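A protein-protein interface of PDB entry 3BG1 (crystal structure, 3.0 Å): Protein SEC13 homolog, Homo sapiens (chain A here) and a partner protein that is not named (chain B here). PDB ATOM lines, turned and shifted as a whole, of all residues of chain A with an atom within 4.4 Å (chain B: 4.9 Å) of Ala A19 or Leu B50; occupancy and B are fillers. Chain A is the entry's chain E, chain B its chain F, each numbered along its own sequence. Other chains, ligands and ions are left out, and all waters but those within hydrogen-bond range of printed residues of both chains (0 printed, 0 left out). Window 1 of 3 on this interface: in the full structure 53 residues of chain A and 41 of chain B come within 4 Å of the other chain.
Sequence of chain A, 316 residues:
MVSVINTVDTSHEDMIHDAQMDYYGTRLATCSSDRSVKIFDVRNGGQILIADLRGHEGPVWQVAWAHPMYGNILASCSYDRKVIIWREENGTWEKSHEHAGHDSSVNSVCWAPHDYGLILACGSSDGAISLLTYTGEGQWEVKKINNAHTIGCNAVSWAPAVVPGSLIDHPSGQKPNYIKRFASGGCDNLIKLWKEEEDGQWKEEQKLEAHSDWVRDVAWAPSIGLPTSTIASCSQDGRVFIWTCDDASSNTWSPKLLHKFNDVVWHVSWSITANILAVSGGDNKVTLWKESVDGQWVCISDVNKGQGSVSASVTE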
ATOM      1  N   ASP A  18     -27.754 -21.010  -1.434  1.00  0.00           N
ATOM      2  CA  ASP A  18     -26.615 -20.281  -1.966  1.00  0.00           C
ATOM      3  C   ASP A  18     -26.802 -18.809  -1.656  1.00  0.00           C
ATOM      4  O   ASP A  18     -27.935 -18.332  -1.548  1.00  0.00           O
ATOM      5  CB  ASP A  18     -26.528 -20.476  -3.485  1.00  0.00           C
ATOM      6  CG  ASP A  18     -25.233 -19.945  -4.075  1.00  0.00           C
ATOM      7  OD1 ASP A  18     -24.867 -18.786  -3.800  1.00  0.00           O
ATOM      8  OD2 ASP A  18     -24.579 -20.692  -4.826  1.00  0.00           O
ATOM      9  N   ALA A  19     -25.694 -18.093  -1.493  1.00  0.00           N
ATOM     10  CA  ALA A  19     -25.747 -16.656  -1.235  1.00  0.00           C
ATOM     11  C   ALA A  19     -24.459 -16.043  -1.776  1.00  0.00           C
ATOM     12  O   ALA A  19     -23.369 -16.446  -1.387  1.00  0.00           O
ATOM     13  CB  ALA A  19     -25.887 -16.391   0.251  1.00  0.00           C
ATOM     14  N   GLN A  20     -24.581 -15.069  -2.671  1.00  0.00           N
ATOM     15  CA  GLN A  20     -23.395 -14.476  -3.272  1.00  0.00           C
ATOM     16  C   GLN A  20     -23.286 -12.968  -3.125  1.00  0.00           C
ATOM     17  O   GLN A  20     -24.233 -12.217  -3.363  1.00  0.00           O
ATOM     18  CB  GLN A  20     -23.318 -14.854  -4.765  1.00  0.00           C
ATOM     19  CG  GLN A  20     -22.094 -14.296  -5.496  1.00  0.00           C
ATOM     20  CD  GLN A  20     -22.188 -14.413  -7.011  1.00  0.00           C
ATOM     21  OE1 GLN A  20     -23.278 -14.492  -7.572  1.00  0.00           O
ATOM     22  NE2 GLN A  20     -21.041 -14.394  -7.679  1.00  0.00           N
ATOM     23  N   MET A  21     -22.093 -12.537  -2.754  1.00  0.00           N
ATOM     24  CA  MET A  21     -21.812 -11.134  -2.576  1.00  0.00           C
ATOM     25  C   MET A  21     -21.884 -10.404  -3.909  1.00  0.00           C
ATOM     26  O   MET A  21     -21.619 -10.973  -4.946  1.00  0.00           O
ATOM     27  CB  MET A  21     -20.421 -10.989  -1.998  1.00  0.00           C
ATOM     28  CG  MET A  21     -20.048  -9.591  -1.641  1.00  0.00           C
ATOM     29  SD  MET A  21     -20.305  -9.380   0.104  1.00  0.00           S
ATOM     30  CE  MET A  21     -19.413 -10.809   0.740  1.00  0.00           C
ATOM     31  N   LEU A  28     -25.483  -8.430  -0.713  1.00  0.00           N
ATOM     32  CA  LEU A  28     -25.289  -9.849  -0.467  1.00  0.00           C
ATOM     33  C   LEU A  28     -26.606 -10.571  -0.660  1.00  0.00           C
ATOM     34  O   LEU A  28     -27.329 -10.781   0.296  1.00  0.00           O
ATOM     35  CB  LEU A  28     -24.826 -10.110   0.958  1.00  0.00           C
ATOM     36  CG  LEU A  28     -24.445 -11.589   1.032  1.00  0.00           C
ATOM     37  CD1 LEU A  28     -22.943 -11.610   0.827  1.00  0.00           C
ATOM     38  CD2 LEU A  28     -24.815 -12.290   2.339  1.00  0.00           C
ATOM     39  N   ALA A  29     -26.930 -10.970  -1.881  1.00  0.00           N
ATOM     40  CA  ALA A  29     -28.191 -11.662  -2.106  1.00  0.00           C
ATOM     41  C   ALA A  29     -28.191 -13.062  -1.497  1.00  0.00           C
ATOM     42  O   ALA A  29     -27.146 -13.706  -1.376  1.00  0.00           O
ATOM     43  CB  ALA A  29     -28.489 -11.733  -3.597  1.00  0.00           C
ATOM     44  N   THR A  30     -29.377 -13.518  -1.110  1.00  0.00           N
ATOM     45  CA  THR A  30     -29.534 -14.831  -0.512  1.00  0.00           C
ATOM     46  C   THR A  30     -30.852 -15.464  -0.887  1.00  0.00           C
ATOM     47  O   THR A  30     -31.782 -14.785  -1.322  1.00  0.00           O
ATOM     48  CB  THR A  30     -29.474 -14.750   1.002  1.00  0.00           C
ATOM     49  OG1 THR A  30     -28.205 -14.204   1.378  1.00  0.00           O
ATOM     50  CG2 THR A  30     -29.634 -16.122   1.618  1.00  0.00           C
ATOM     51  N   PHE B  40     -22.120 -25.184   2.425  1.00  0.00           N
ATOM     52  CA  PHE B  40     -21.677 -24.511   1.209  1.00  0.00           C
ATOM     53  C   PHE B  40     -20.792 -23.314   1.528  1.00  0.00           C
ATOM     54  O   PHE B  40     -20.808 -22.796   2.638  1.00  0.00           O
ATOM     55  CB  PHE B  40     -22.894 -24.044   0.412  1.00  0.00           C
ATOM     56  CG  PHE B  40     -23.441 -22.735   0.882  1.00  0.00           C
ATOM     57  CD1 PHE B  40     -23.001 -21.541   0.320  1.00  0.00           C
ATOM     58  CD2 PHE B  40     -24.346 -22.689   1.933  1.00  0.00           C
ATOM     59  CE1 PHE B  40     -23.456 -20.328   0.797  1.00  0.00           C
ATOM     60  CE2 PHE B  40     -24.802 -21.476   2.421  1.00  0.00           C
ATOM     61  CZ  PHE B  40     -24.356 -20.294   1.850  1.00  0.00           C
ATOM     62  N   ALA B  41     -20.034 -22.855   0.546  1.00  0.00           N
ATOM     63  CA  ALA B  41     -19.151 -21.717   0.764  1.00  0.00           C
ATOM     64  C   ALA B  41     -18.583 -21.236  -0.564  1.00  0.00           C
ATOM     65  O   ALA B  41     -18.189 -22.040  -1.401  1.00  0.00           O
ATOM     66  CB  ALA B  41     -18.025 -22.119   1.705  1.00  0.00           C
ATOM     67  N   LYS B  42     -18.516 -19.929  -0.753  1.00  0.00           N
ATOM     68  CA  LYS B  42     -18.021 -19.395  -2.014  1.00  0.00           C
ATOM     69  C   LYS B  42     -17.168 -18.145  -1.875  1.00  0.00           C
ATOM     70  O   LYS B  42     -17.619 -17.196  -1.284  1.00  0.00           O
ATOM     71  CB  LYS B  42     -19.207 -19.052  -2.918  1.00  0.00           C
ATOM     72  CG  LYS B  42     -19.982 -20.243  -3.419  1.00  0.00           C
ATOM     73  CD  LYS B  42     -21.117 -19.811  -4.330  1.00  0.00           C
ATOM     74  CE  LYS B  42     -21.718 -21.009  -5.052  1.00  0.00           C
ATOM     75  NZ  LYS B  42     -22.504 -20.611  -6.261  1.00  0.00           N
ATOM     76  N   SER B  44     -15.574 -14.468  -2.782  1.00  0.00           N
ATOM     77  CA  SER B  44     -16.137 -13.350  -3.547  1.00  0.00           C
ATOM     78  C   SER B  44     -15.093 -12.401  -4.055  1.00  0.00           C
ATOM     79  O   SER B  44     -13.940 -12.468  -3.662  1.00  0.00           O
ATOM     80  CB  SER B  44     -17.170 -12.572  -2.740  1.00  0.00           C
ATOM     81  OG  SER B  44     -18.417 -13.253  -2.749  1.00  0.00           O
ATOM     82  N   MET B  48     -13.257 -12.410  -0.073  1.00  0.00           N
ATOM     83  CA  MET B  48     -13.795 -12.895   1.190  1.00  0.00           C
ATOM     84  C   MET B  48     -14.679 -14.072   0.864  1.00  0.00           C
ATOM     85  O   MET B  48     -15.278 -14.118  -0.201  1.00  0.00           O
ATOM     86  CB  MET B  48     -14.602 -11.824   1.911  1.00  0.00           C
ATOM     87  CG  MET B  48     -15.012 -10.654   1.062  1.00  0.00           C
ATOM     88  SD  MET B  48     -15.175  -9.243   2.160  1.00  0.00           S
ATOM     89  CE  MET B  48     -13.462  -8.976   2.582  1.00  0.00           C
ATOM     90  N   LEU B  49     -14.751 -15.018   1.788  1.00  0.00           N
ATOM     91  CA  LEU B  49     -15.533 -16.232   1.622  1.00  0.00           C
ATOM     92  C   LEU B  49     -16.843 -16.205   2.441  1.00  0.00           C
ATOM     93  O   LEU B  49     -16.858 -15.677   3.527  1.00  0.00           O
ATOM     94  CB  LEU B  49     -14.638 -17.417   2.043  1.00  0.00           C
ATOM     95  CG  LEU B  49     -15.284 -18.622   2.762  1.00  0.00           C
ATOM     96  CD1 LEU B  49     -16.461 -19.244   1.944  1.00  0.00           C
ATOM     97  CD2 LEU B  49     -14.193 -19.665   3.026  1.00  0.00           C
ATOM     98  N   LEU B  50     -17.936 -16.781   1.956  1.00  0.00           N
ATOM     99  CA  LEU B  50     -19.148 -16.741   2.751  1.00  0.00           C
ATOM    100  C   LEU B  50     -19.573 -18.110   3.276  1.00  0.00           C
ATOM    101  O   LEU B  50     -20.310 -18.837   2.615  1.00  0.00           O
ATOM    102  CB  LEU B  50     -20.281 -16.115   1.942  1.00  0.00           C
ATOM    103  CG  LEU B  50     -19.810 -15.052   0.927  1.00  0.00           C
ATOM    104  CD1 LEU B  50     -21.039 -14.273   0.397  1.00  0.00           C
ATOM    105  CD2 LEU B  50     -18.752 -14.096   1.519  1.00  0.00           C
ATOM    106  N   THR B  51     -19.131 -18.465   4.477  1.00  0.00           N
ATOM    107  CA  THR B  51     -19.512 -19.754   5.068  1.00  0.00           C
ATOM    108  C   THR B  51     -20.912 -19.654   5.686  1.00  0.00           C
ATOM    109  O   THR B  51     -21.349 -18.563   6.013  1.00  0.00           O
ATOM    110  CB  THR B  51     -18.536 -20.136   6.190  1.00  0.00           C
ATOM    111  OG1 THR B  51     -17.193 -20.039   5.704  1.00  0.00           O
ATOM    112  CG2 THR B  51     -18.814 -21.552   6.686  1.00  0.00           C
ATOM    113  N   LYS B  52     -21.630 -20.760   5.848  1.00  0.00           N
ATOM    114  CA  LYS B  52     -22.943 -20.661   6.487  1.00  0.00           C
ATOM    115  C   LYS B  52     -22.778 -21.112   7.960  1.00  0.00           C
ATOM    116  O   LYS B  52     -22.341 -22.242   8.209  1.00  0.00           O
ATOM    117  CB  LYS B  52     -23.951 -21.524   5.746  1.00  0.00           C
ATOM    118  CG  LYS B  52     -24.142 -22.882   6.343  1.00  0.00           C
ATOM    119  CD  LYS B  52     -25.513 -23.376   5.979  1.00  0.00           C
ATOM    120  CE  LYS B  52     -26.134 -24.178   7.107  1.00  0.00           C
ATOM    121  NZ  LYS B  52     -27.514 -24.581   6.722  1.00  0.00           N
ATOM    122  N   VAL B  60     -25.225 -16.142   6.837  1.00  0.00           N
ATOM    123  CA  VAL B  60     -24.128 -16.034   5.877  1.00  0.00           C
ATOM    124  C   VAL B  60     -22.837 -15.520   6.531  1.00  0.00           C
ATOM    125  O   VAL B  60     -22.514 -14.336   6.454  1.00  0.00           O
ATOM    126  CB  VAL B  60     -24.499 -15.086   4.691  1.00  0.00           C
ATOM    127  CG1 VAL B  60     -23.282 -14.848   3.807  1.00  0.00           C
ATOM    128  CG2 VAL B  60     -25.618 -15.692   3.860  1.00  0.00           C
ATOM    129  N   SER B  61     -22.095 -16.417   7.170  1.00  0.00           N
ATOM    130  CA  SER B  61     -20.846 -16.036   7.816  1.00  0.00           C
ATOM    131  C   SER B  61     -19.836 -15.575   6.800  1.00  0.00           C
ATOM    132  O   SER B  61     -19.090 -16.364   6.228  1.00  0.00           O
ATOM    133  CB  SER B  61     -20.249 -17.198   8.614  1.00  0.00           C
ATOM    134  OG  SER B  61     -20.926 -17.369   9.837  1.00  0.00           O
ATOM    135  N   ILE B  62     -19.828 -14.279   6.577  1.00  0.00           N
ATOM    136  CA  ILE B  62     -18.897 -13.663   5.658  1.00  0.00           C
ATOM    137  C   ILE B  62     -17.446 -13.529   6.227  1.00  0.00           C
ATOM    138  O   ILE B  62     -16.887 -12.417   6.213  1.00  0.00           O
ATOM    139  CB  ILE B  62     -19.441 -12.276   5.294  1.00  0.00           C
ATOM    140  CG1 ILE B  62     -20.832 -12.449   4.684  1.00  0.00           C
ATOM    141  CG2 ILE B  62     -18.461 -11.504   4.400  1.00  0.00           C
ATOM    142  CD1 ILE B  62     -21.266 -11.287   3.720  1.00  0.00           C
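OD2 of Asp A18 lies within salt-bridge range of NZ of Lys B42 (2.5 Å).
Ala A19 touches three residues of chain B. Of the printed residues of chain A, Leu B50 touches Ala A19, Met A21 and Leu A28. Printed residues of chain A within 4 Å of Ser B44: Met A21 (3.1 Å). Of the printed residues of chain B, Asp A18 touches Lys B42 (2.5 Å). Printed residues of chain B within 4 Å of Thr A30: Val B60. Printed residues of chain B within 4 Å of Leu A28: Leu B50, Val B60 and Ile B62. Ala B41 touches none of the printed residues of chain A.
The backbone carbonyl oxygen (O) of Lys B42 lies within hydrogen-bond range of the backbone NH (N) of Leu B50.
Hydrophobic or aromatic side chains of chain B that line the printed part of chain A: Phe B40, Leu B50, Val B60 and Ile B62. Of the 7 printed residues of chain A, 5 touch a printed residue of chain B. Among the printed residues, Asp or Glu carboxylates within 4 Å of a Lys or Arg side-chain nitrogen of the other chain: Asp A18 with Lys B42 (2.5 Å).
N of Ala A19 touches CE1 of Phe B40 (3.9 Å). Ala A19 touches Leu B50. CB of Ala A19 touches CG2 of Val B60, at 3.7 Å. Met A21 touches Ser B44. Leu B50 touches Met A21 (CD2 to CE, 3.4 Å). Met A21 touches Ile B62. CD1 of Leu A28 touches CD1 of Leu B50 (3.3 Å). Val B60 touches Leu A28 (CG1 to CD2, 3.3 Å). Ile B62 touches Leu A28. Thr A30 touches Val B60 (OG1 to CG2, 3.9 Å).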
